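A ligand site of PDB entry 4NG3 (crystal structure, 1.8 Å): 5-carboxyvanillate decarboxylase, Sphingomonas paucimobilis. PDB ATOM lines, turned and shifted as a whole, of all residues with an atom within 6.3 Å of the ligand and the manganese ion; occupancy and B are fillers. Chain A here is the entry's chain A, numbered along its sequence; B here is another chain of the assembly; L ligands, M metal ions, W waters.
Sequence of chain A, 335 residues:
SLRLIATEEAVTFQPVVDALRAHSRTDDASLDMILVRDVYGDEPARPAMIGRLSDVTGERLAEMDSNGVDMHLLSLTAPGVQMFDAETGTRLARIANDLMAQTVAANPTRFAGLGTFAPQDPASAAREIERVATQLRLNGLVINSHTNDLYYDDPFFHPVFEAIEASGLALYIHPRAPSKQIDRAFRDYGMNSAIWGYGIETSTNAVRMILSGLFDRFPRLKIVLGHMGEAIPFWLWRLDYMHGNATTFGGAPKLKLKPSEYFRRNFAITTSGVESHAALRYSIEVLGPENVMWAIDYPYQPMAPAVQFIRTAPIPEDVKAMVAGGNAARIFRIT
O1 of the ligand lies close to OH of Tyr 300.
An oxygen (O3) of the ligand is in salt-bridge range of the guanidinium group of Arg 46, 2.8 Å away.
A ring nitrogen (NE2) of His 227 sits at hydrogen-bond distance from an oxygen (O6) of the ligand, 3.2 Å away.
An oxygen (O6) of the ligand is in hydrogen-bond range of the guanidinium group (NH2) of Arg 238 of chain B (3.0 Å).
A ring nitrogen (NE2) of His 227 is in hydrogen-bond range of the side-chain carboxylate of Asp 297 (3.1 Å).
A ring nitrogen (NE2) of His 227 sits close to the side-chain carboxylate of Glu 8, 3.3 Å away.
The backbone carbonyl oxygen (O) of Ser 193 lies within hydrogen-bond range of the backbone NH (N) of Tyr 198 (3.0 Å).
NE2 of His 227 lies close to NH2 of Arg 238 of chain B, 3.4 Å away.
O of Ala 194 sits at hydrogen-bond distance from NE of Arg 238 of chain B (3.4 Å).
The side-chain carboxylate of Glu 8 is in hydrogen-bond range of the side-chain hydroxyl of Ser 272, at 2.6 Å.
The side-chain hydroxyl (OH) of Tyr 300 is in hydrogen-bond range of the side-chain hydroxyl (OG1) of Thr 77 (2.7 Å).
N of His 227 sits at hydrogen-bond distance from OG of Ser 272, at 2.9 Å.
Residues that only touch the ligand: Ala 78, Leu 35, Thr 77, Ser 193, Asn 245 of chain B, Ala 194, Tyr 198 and Met 242 of chain B.
The nearest printed residue that does not touch the ligand is Pro 175 (4.8 Å).
Three residues have an atom within 4 Å of the manganese ion: Glu 8, His 174 and Asp 297.
The manganese ion is bound by an oxygen (O5) of the ligand (1.9 Å), an oxygen (O4) of the ligand (2.1 Å), the side-chain carboxylate of Glu 8 (2.2 Å), a ring nitrogen (NE2) of His 174 (2.2 Å), water W2 (2.2 Å) and the side-chain carboxylate of Asp 297 (2.3 Å).
Water W1 lies within hydrogen-bond range of O2 of the ligand (2.6 Å), ND2 of Asn 245 of chain B (2.8 Å), O of Tyr 300 (2.9 Å) and NH2 of Arg 46 (3.5 Å).
Water W6 lies within hydrogen-bond range of OH of Tyr 198 (2.6 Å), O3 of the ligand (2.7 Å) and OG of Ser 193 (2.7 Å).
Water W3 lies within hydrogen-bond range of O2 of the ligand (2.7 Å), ND2 of Asn 245 of chain B (2.9 Å) and OG of Ser 193 (3.0 Å).
Water W5 lies within hydrogen-bond range of the side-chain hydroxyl (OG1) of Thr 77 (2.7 Å), an oxygen (O1) of the ligand (3.0 Å) and the backbone NH (N) of Ala 78 (3.0 Å).
Water W4 lies within hydrogen-bond range of OD2 of Asp 297, NE2 of Gln 301, NH1 of Arg 238 of chain B and O6 of the ligand.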
ATOM      1  N   GLU A   8       0.670  -9.770  -7.039  1.00  0.00           N
ATOM      2  CA  GLU A   8       0.980  -8.645  -6.148  1.00  0.00           C
ATOM      3  C   GLU A   8       0.837  -9.041  -4.681  1.00  0.00           C
ATOM      4  O   GLU A   8       0.057  -8.456  -3.933  1.00  0.00           O
ATOM      5  CB  GLU A   8       0.117  -7.402  -6.455  1.00  0.00           C
ATOM      6  CG  GLU A   8       0.667  -6.108  -5.826  1.00  0.00           C
ATOM      7  CD  GLU A   8      -0.267  -4.913  -6.016  1.00  0.00           C
ATOM      8  OE1 GLU A   8      -0.596  -4.565  -7.171  1.00  0.00           O
ATOM      9  OE2 GLU A   8      -0.685  -4.323  -4.992  1.00  0.00           O
ATOM     10  N   ALA A  10       2.031  -9.472  -0.999  1.00  0.00           N
ATOM     11  CA  ALA A  10       2.960  -8.819  -0.093  1.00  0.00           C
ATOM     12  C   ALA A  10       3.516  -9.769   0.948  1.00  0.00           C
ATOM     13  O   ALA A  10       2.832 -10.661   1.424  1.00  0.00           O
ATOM     14  CB  ALA A  10       2.283  -7.612   0.577  1.00  0.00           C
ATOM     15  N   LEU A  35       0.655   4.620   7.564  1.00  0.00           N
ATOM     16  CA  LEU A  35       0.750   3.167   7.482  1.00  0.00           C
ATOM     17  C   LEU A  35       1.782   2.622   8.468  1.00  0.00           C
ATOM     18  O   LEU A  35       1.526   1.640   9.172  1.00  0.00           O
ATOM     19  CB  LEU A  35       1.139   2.749   6.049  1.00  0.00           C
ATOM     20  CG  LEU A  35       1.611   1.309   5.871  1.00  0.00           C
ATOM     21  CD1 LEU A  35       0.421   0.368   6.000  1.00  0.00           C
ATOM     22  CD2 LEU A  35       2.302   1.125   4.510  1.00  0.00           C
ATOM     23  N   TYR A  40       3.426  -0.995  11.991  1.00  0.00           N
ATOM     24  CA  TYR A  40       4.726  -1.266  12.609  1.00  0.00           C
ATOM     25  C   TYR A  40       4.952  -0.524  13.924  1.00  0.00           C
ATOM     26  O   TYR A  40       5.989  -0.674  14.558  1.00  0.00           O
ATOM     27  CB  TYR A  40       5.854  -0.954  11.615  1.00  0.00           C
ATOM     28  CG  TYR A  40       5.703  -1.688  10.316  1.00  0.00           C
ATOM     29  CD1 TYR A  40       6.183  -2.982  10.168  1.00  0.00           C
ATOM     30  CD2 TYR A  40       5.064  -1.100   9.234  1.00  0.00           C
ATOM     31  CE1 TYR A  40       6.031  -3.666   8.986  1.00  0.00           C
ATOM     32  CE2 TYR A  40       4.900  -1.780   8.040  1.00  0.00           C
ATOM     33  CZ  TYR A  40       5.394  -3.063   7.923  1.00  0.00           C
ATOM     34  OH  TYR A  40       5.248  -3.755   6.742  1.00  0.00           O
ATOM     35  N   ARG A  46      -3.524  -1.671  13.455  1.00  0.00           N
ATOM     36  CA  ARG A  46      -3.655  -2.880  12.668  1.00  0.00           C
ATOM     37  C   ARG A  46      -2.661  -3.923  13.164  1.00  0.00           C
ATOM     38  O   ARG A  46      -1.716  -4.273  12.454  1.00  0.00           O
ATOM     39  CB  ARG A  46      -3.413  -2.557  11.186  1.00  0.00           C
ATOM     40  CG  ARG A  46      -4.349  -1.489  10.643  1.00  0.00           C
ATOM     41  CD  ARG A  46      -3.927  -1.006   9.266  1.00  0.00           C
ATOM     42  NE  ARG A  46      -4.296  -1.925   8.182  1.00  0.00           N
ATOM     43  CZ  ARG A  46      -4.077  -1.682   6.895  1.00  0.00           C
ATOM     44  NH1 ARG A  46      -3.491  -0.542   6.532  1.00  0.00           N
ATOM     45  NH2 ARG A  46      -4.435  -2.553   5.950  1.00  0.00           N
ATOM     46  N   THR A  77       6.666  -5.751   1.035  1.00  0.00           N
ATOM     47  CA  THR A  77       5.505  -4.869   1.079  1.00  0.00           C
ATOM     48  C   THR A  77       5.935  -3.407   1.120  1.00  0.00           C
ATOM     49  O   THR A  77       7.028  -3.088   1.593  1.00  0.00           O
ATOM     50  CB  THR A  77       4.639  -5.179   2.309  1.00  0.00           C
ATOM     51  OG1 THR A  77       3.402  -4.459   2.228  1.00  0.00           O
ATOM     52  CG2 THR A  77       5.364  -4.795   3.609  1.00  0.00           C
ATOM     53  N   ALA A  78       5.072  -2.535   0.619  1.00  0.00           N
ATOM     54  CA  ALA A  78       5.347  -1.107   0.708  1.00  0.00           C
ATOM     55  C   ALA A  78       5.482  -0.729   2.173  1.00  0.00           C
ATOM     56  O   ALA A  78       4.801  -1.294   3.028  1.00  0.00           O
ATOM     57  CB  ALA A  78       4.223  -0.308   0.037  1.00  0.00           C
ATOM     58  N   PRO A  79       6.370   0.238   2.477  1.00  0.00           N
ATOM     59  CA  PRO A  79       7.169   1.070   1.573  1.00  0.00           C
ATOM     60  C   PRO A  79       8.547   0.481   1.266  1.00  0.00           C
ATOM     61  O   PRO A  79       9.486   1.233   0.926  1.00  0.00           O
ATOM     62  CB  PRO A  79       7.335   2.357   2.378  1.00  0.00           C
ATOM     63  CG  PRO A  79       7.435   1.859   3.795  1.00  0.00           C
ATOM     64  CD  PRO A  79       6.555   0.636   3.885  1.00  0.00           C
ATOM     65  N   HIS A 174       4.901  -0.563  -7.465  1.00  0.00           N
ATOM     66  CA  HIS A 174       3.803  -0.680  -6.513  1.00  0.00           C
ATOM     67  C   HIS A 174       3.544   0.686  -5.865  1.00  0.00           C
ATOM     68  O   HIS A 174       4.436   1.549  -5.846  1.00  0.00           O
ATOM     69  CB  HIS A 174       4.181  -1.740  -5.470  1.00  0.00           C
ATOM     70  CG  HIS A 174       3.104  -2.022  -4.463  1.00  0.00           C
ATOM     71  ND1 HIS A 174       2.915  -1.258  -3.340  1.00  0.00           N
ATOM     72  CD2 HIS A 174       2.171  -3.004  -4.417  1.00  0.00           C
ATOM     73  CE1 HIS A 174       1.894  -1.733  -2.646  1.00  0.00           C
ATOM     74  NE2 HIS A 174       1.431  -2.794  -3.274  1.00  0.00           N
ATOM     75  N   PRO A 175       2.334   0.912  -5.343  1.00  0.00           N
ATOM     76  CA  PRO A 175       2.119   2.220  -4.707  1.00  0.00           C
ATOM     77  C   PRO A 175       2.834   2.395  -3.373  1.00  0.00           C
ATOM     78  O   PRO A 175       3.253   1.422  -2.735  1.00  0.00           O
ATOM     79  CB  PRO A 175       0.613   2.218  -4.417  1.00  0.00           C
ATOM     80  CG  PRO A 175       0.034   1.298  -5.420  1.00  0.00           C
ATOM     81  CD  PRO A 175       1.053   0.188  -5.551  1.00  0.00           C
ATOM     82  N   SER A 193      -4.172   6.385   1.621  1.00  0.00           N
ATOM     83  CA  SER A 193      -3.990   4.958   1.364  1.00  0.00           C
ATOM     84  C   SER A 193      -4.579   4.496   0.033  1.00  0.00           C
ATOM     85  O   SER A 193      -4.731   5.267  -0.916  1.00  0.00           O
ATOM     86  CB  SER A 193      -4.587   4.170   2.545  1.00  0.00           C
ATOM     87  OG  SER A 193      -4.242   2.780   2.502  1.00  0.00           O
ATOM     88  N   ALA A 194      -4.909   3.204  -0.011  1.00  0.00           N
ATOM     89  CA  ALA A 194      -5.391   2.561  -1.238  1.00  0.00           C
ATOM     90  C   ALA A 194      -6.680   3.155  -1.808  1.00  0.00           C
ATOM     91  O   ALA A 194      -6.915   3.097  -3.035  1.00  0.00           O
ATOM     92  CB  ALA A 194      -5.581   1.074  -0.992  1.00  0.00           C
ATOM     93  N   TYR A 198      -2.891   6.146  -3.155  1.00  0.00           N
ATOM     94  CA  TYR A 198      -1.977   5.190  -3.791  1.00  0.00           C
ATOM     95  C   TYR A 198      -2.053   5.285  -5.317  1.00  0.00           C
ATOM     96  O   TYR A 198      -1.029   5.282  -5.994  1.00  0.00           O
ATOM     97  CB  TYR A 198      -2.295   3.748  -3.350  1.00  0.00           C
ATOM     98  CG  TYR A 198      -1.707   3.349  -2.004  1.00  0.00           C
ATOM     99  CD1 TYR A 198      -1.118   4.288  -1.173  1.00  0.00           C
ATOM    100  CD2 TYR A 198      -1.718   2.017  -1.592  1.00  0.00           C
ATOM    101  CE1 TYR A 198      -0.557   3.928   0.056  1.00  0.00           C
ATOM    102  CE2 TYR A 198      -1.169   1.638  -0.362  1.00  0.00           C
ATOM    103  CZ  TYR A 198      -0.602   2.597   0.455  1.00  0.00           C
ATOM    104  OH  TYR A 198      -0.054   2.241   1.673  1.00  0.00           O
ATOM    105  N   HIS A 227      -3.610  -2.534  -9.627  1.00  0.00           N
ATOM    106  CA  HIS A 227      -4.846  -1.751  -9.492  1.00  0.00           C
ATOM    107  C   HIS A 227      -5.391  -1.306 -10.847  1.00  0.00           C
ATOM    108  O   HIS A 227      -5.765  -0.148 -11.051  1.00  0.00           O
ATOM    109  CB  HIS A 227      -4.614  -0.600  -8.510  1.00  0.00           C
ATOM    110  CG  HIS A 227      -3.819  -1.044  -7.332  1.00  0.00           C
ATOM    111  ND1 HIS A 227      -2.515  -0.650  -7.107  1.00  0.00           N
ATOM    112  CD2 HIS A 227      -4.105  -1.938  -6.355  1.00  0.00           C
ATOM    113  CE1 HIS A 227      -2.054  -1.246  -6.031  1.00  0.00           C
ATOM    114  NE2 HIS A 227      -2.992  -2.036  -5.546  1.00  0.00           N
ATOM    115  N   SER A 272      -5.025  -6.276  -9.217  1.00  0.00           N
ATOM    116  CA  SER A 272      -5.042  -6.178  -7.755  1.00  0.00           C
ATOM    117  C   SER A 272      -6.005  -5.118  -7.262  1.00  0.00           C
ATOM    118  O   SER A 272      -5.961  -3.966  -7.708  1.00  0.00           O
ATOM    119  CB  SER A 272      -3.643  -5.899  -7.220  1.00  0.00           C
ATOM    120  OG  SER A 272      -3.069  -4.793  -7.883  1.00  0.00           O
ATOM    121  N   GLY A 273      -6.909  -5.515  -6.371  1.00  0.00           N
ATOM    122  CA  GLY A 273      -7.825  -4.572  -5.744  1.00  0.00           C
ATOM    123  C   GLY A 273      -8.858  -3.951  -6.666  1.00  0.00           C
ATOM    124  O   GLY A 273      -9.555  -3.009  -6.269  1.00  0.00           O
ATOM    125  N   ASP A 297      -3.459  -9.207  -4.131  1.00  0.00           N
ATOM    126  CA  ASP A 297      -3.052  -8.158  -3.174  1.00  0.00           C
ATOM    127  C   ASP A 297      -3.185  -8.653  -1.719  1.00  0.00           C
ATOM    128  O   ASP A 297      -3.494  -7.879  -0.810  1.00  0.00           O
ATOM    129  CB  ASP A 297      -3.868  -6.864  -3.380  1.00  0.00           C
ATOM    130  CG  ASP A 297      -3.037  -5.595  -3.246  1.00  0.00           C
ATOM    131  OD1 ASP A 297      -1.960  -5.631  -2.617  1.00  0.00           O
ATOM    132  OD2 ASP A 297      -3.479  -4.550  -3.780  1.00  0.00           O
ATOM    133  N   TYR A 300      -3.618  -7.666   2.104  1.00  0.00           N
ATOM    134  CA  TYR A 300      -4.445  -6.460   2.165  1.00  0.00           C
ATOM    135  C   TYR A 300      -5.827  -6.702   1.568  1.00  0.00           C
ATOM    136  O   TYR A 300      -6.774  -5.959   1.855  1.00  0.00           O
ATOM    137  CB  TYR A 300      -3.739  -5.281   1.499  1.00  0.00           C
ATOM    138  CG  TYR A 300      -2.383  -5.016   2.111  1.00  0.00           C
ATOM    139  CD1 TYR A 300      -2.279  -4.482   3.401  1.00  0.00           C
ATOM    140  CD2 TYR A 300      -1.209  -5.328   1.431  1.00  0.00           C
ATOM    141  CE1 TYR A 300      -1.048  -4.257   3.974  1.00  0.00           C
ATOM    142  CE2 TYR A 300       0.036  -5.106   2.006  1.00  0.00           C
ATOM    143  CZ  TYR A 300       0.101  -4.562   3.281  1.00  0.00           C
ATOM    144  OH  TYR A 300       1.317  -4.331   3.873  1.00  0.00           O
ATOM    145  N   GLN A 301      -5.939  -7.734   0.729  1.00  0.00           N
ATOM    146  CA  GLN A 301      -7.226  -8.214   0.210  1.00  0.00           C
ATOM    147  C   GLN A 301      -7.294  -9.714   0.458  1.00  0.00           C
ATOM    148  O   GLN A 301      -6.263 -10.388   0.446  1.00  0.00           O
ATOM    149  CB  GLN A 301      -7.322  -8.002  -1.306  1.00  0.00           C
ATOM    150  CG  GLN A 301      -7.181  -6.570  -1.774  1.00  0.00           C
ATOM    151  CD  GLN A 301      -8.507  -5.948  -2.149  1.00  0.00           C
ATOM    152  OE1 GLN A 301      -9.537  -6.626  -2.186  1.00  0.00           O
ATOM    153  NE2 GLN A 301      -8.481  -4.658  -2.426  1.00  0.00           N
ATOM    154  N   ARG B 238     -12.821   0.000  -6.295  1.00  0.00           N
ATOM    155  CA  ARG B 238     -11.780   0.198  -5.294  1.00  0.00           C
ATOM    156  C   ARG B 238     -12.204   1.224  -4.254  1.00  0.00           C
ATOM    157  O   ARG B 238     -11.959   1.043  -3.048  1.00  0.00           O
ATOM    158  CB  ARG B 238     -10.488   0.618  -5.978  1.00  0.00           C
ATOM    159  CG  ARG B 238      -9.256   0.689  -5.081  1.00  0.00           C
ATOM    160  CD  ARG B 238      -8.060   0.334  -5.927  1.00  0.00           C
ATOM    161  NE  ARG B 238      -6.767   0.674  -5.356  1.00  0.00           N
ATOM    162  CZ  ARG B 238      -6.102  -0.064  -4.471  1.00  0.00           C
ATOM    163  NH1 ARG B 238      -6.632  -1.192  -3.993  1.00  0.00           N
ATOM    164  NH2 ARG B 238      -4.899   0.331  -4.064  1.00  0.00           N
ATOM    165  N   MET B 242     -12.273  -0.123  -0.391  1.00  0.00           N
ATOM    166  CA  MET B 242     -11.374   0.432   0.600  1.00  0.00           C
ATOM    167  C   MET B 242     -12.063   1.385   1.580  1.00  0.00           C
ATOM    168  O   MET B 242     -11.425   1.880   2.510  1.00  0.00           O
ATOM    169  CB  MET B 242     -10.180   1.131  -0.085  1.00  0.00           C
ATOM    170  CG  MET B 242      -9.168   0.177  -0.681  1.00  0.00           C
ATOM    171  SD  MET B 242      -8.555  -0.917   0.608  1.00  0.00           S
ATOM    172  CE  MET B 242      -7.465  -2.020  -0.312  1.00  0.00           C
ATOM    173  N   ASN B 245     -11.811   0.370   5.399  1.00  0.00           N
ATOM    174  CA  ASN B 245     -10.555   0.774   6.001  1.00  0.00           C
ATOM    175  C   ASN B 245     -10.536   2.266   6.343  1.00  0.00           C
ATOM    176  O   ASN B 245     -10.055   2.679   7.406  1.00  0.00           O
ATOM    177  CB  ASN B 245      -9.376   0.456   5.080  1.00  0.00           C
ATOM    178  CG  ASN B 245      -9.073  -1.020   4.989  1.00  0.00           C
ATOM    179  OD1 ASN B 245      -9.571  -1.825   5.788  1.00  0.00           O
ATOM    180  ND2 ASN B 245      -8.231  -1.390   4.040  1.00  0.00           N
ATOM    181  N   PHE B 249      -9.857   2.829  10.314  1.00  0.00           N
ATOM    182  CA  PHE B 249      -8.637   3.383  10.892  1.00  0.00           C
ATOM    183  C   PHE B 249      -8.179   4.677  10.224  1.00  0.00           C
ATOM    184  O   PHE B 249      -7.246   5.322  10.697  1.00  0.00           O
ATOM    185  CB  PHE B 249      -7.507   2.339  10.978  1.00  0.00           C
ATOM    186  CG  PHE B 249      -7.304   1.542   9.718  1.00  0.00           C
ATOM    187  CD1 PHE B 249      -6.505   2.036   8.689  1.00  0.00           C
ATOM    188  CD2 PHE B 249      -7.884   0.295   9.576  1.00  0.00           C
ATOM    189  CE1 PHE B 249      -6.302   1.310   7.535  1.00  0.00           C
ATOM    190  CE2 PHE B 249      -7.689  -0.435   8.421  1.00  0.00           C
ATOM    191  CZ  PHE B 249      -6.895   0.067   7.391  1.00  0.00           C
HETATM  192  C1  LIG L   1      -2.723  -1.515   1.653  1.00  0.00           C
HETATM  193  C2  LIG L   1      -3.147  -1.823   0.356  1.00  0.00           C
HETATM  194  C3  LIG L   1      -1.379  -1.591   1.988  1.00  0.00           C
HETATM  195  C4  LIG L   1      -2.201  -2.215  -0.592  1.00  0.00           C
HETATM  196  C5  LIG L   1      -0.455  -1.984   1.038  1.00  0.00           C
HETATM  197  O1  LIG L   1       0.882  -2.083   1.314  1.00  0.00           O
HETATM  198  C6  LIG L   1      -0.863  -2.304  -0.236  1.00  0.00           C
HETATM  199  C7  LIG L   1      -3.665  -1.082   2.719  1.00  0.00           C
HETATM  200  C8  LIG L   1       1.477  -1.379   2.355  1.00  0.00           C
HETATM  201  O2  LIG L   1      -4.886  -1.352   2.643  1.00  0.00           O
HETATM  202  O3  LIG L   1      -3.210  -0.450   3.711  1.00  0.00           O
HETATM  203  O4  LIG L   1       0.013  -3.062  -0.961  1.00  0.00           O
HETATM  204  N1  LIG L   1      -2.526  -2.241  -1.991  1.00  0.00           N
HETATM  205  O5  LIG L   1      -1.671  -2.700  -2.882  1.00  0.00           O
HETATM  206  O6  LIG L   1      -3.682  -1.817  -2.395  1.00  0.00           O
HETATM  207 MN    MN M   1      -0.377  -4.034  -2.819  1.00  0.00          MN
HETATM  208  O   HOH W   1      -6.438  -3.411   3.235  1.00  0.00           O
HETATM  209  O   HOH W   2       0.820  -5.884  -2.413  1.00  0.00           O
HETATM  210  O   HOH W   3      -6.306   0.777   3.495  1.00  0.00           O
HETATM  211  O   HOH W   4      -5.907  -3.720  -2.886  1.00  0.00           O
HETATM  212  O   HOH W   5       2.551  -3.973  -0.268  1.00  0.00           O
HETATM  213  O   HOH W   6      -1.899   1.859   3.510  1.00  0.00           O
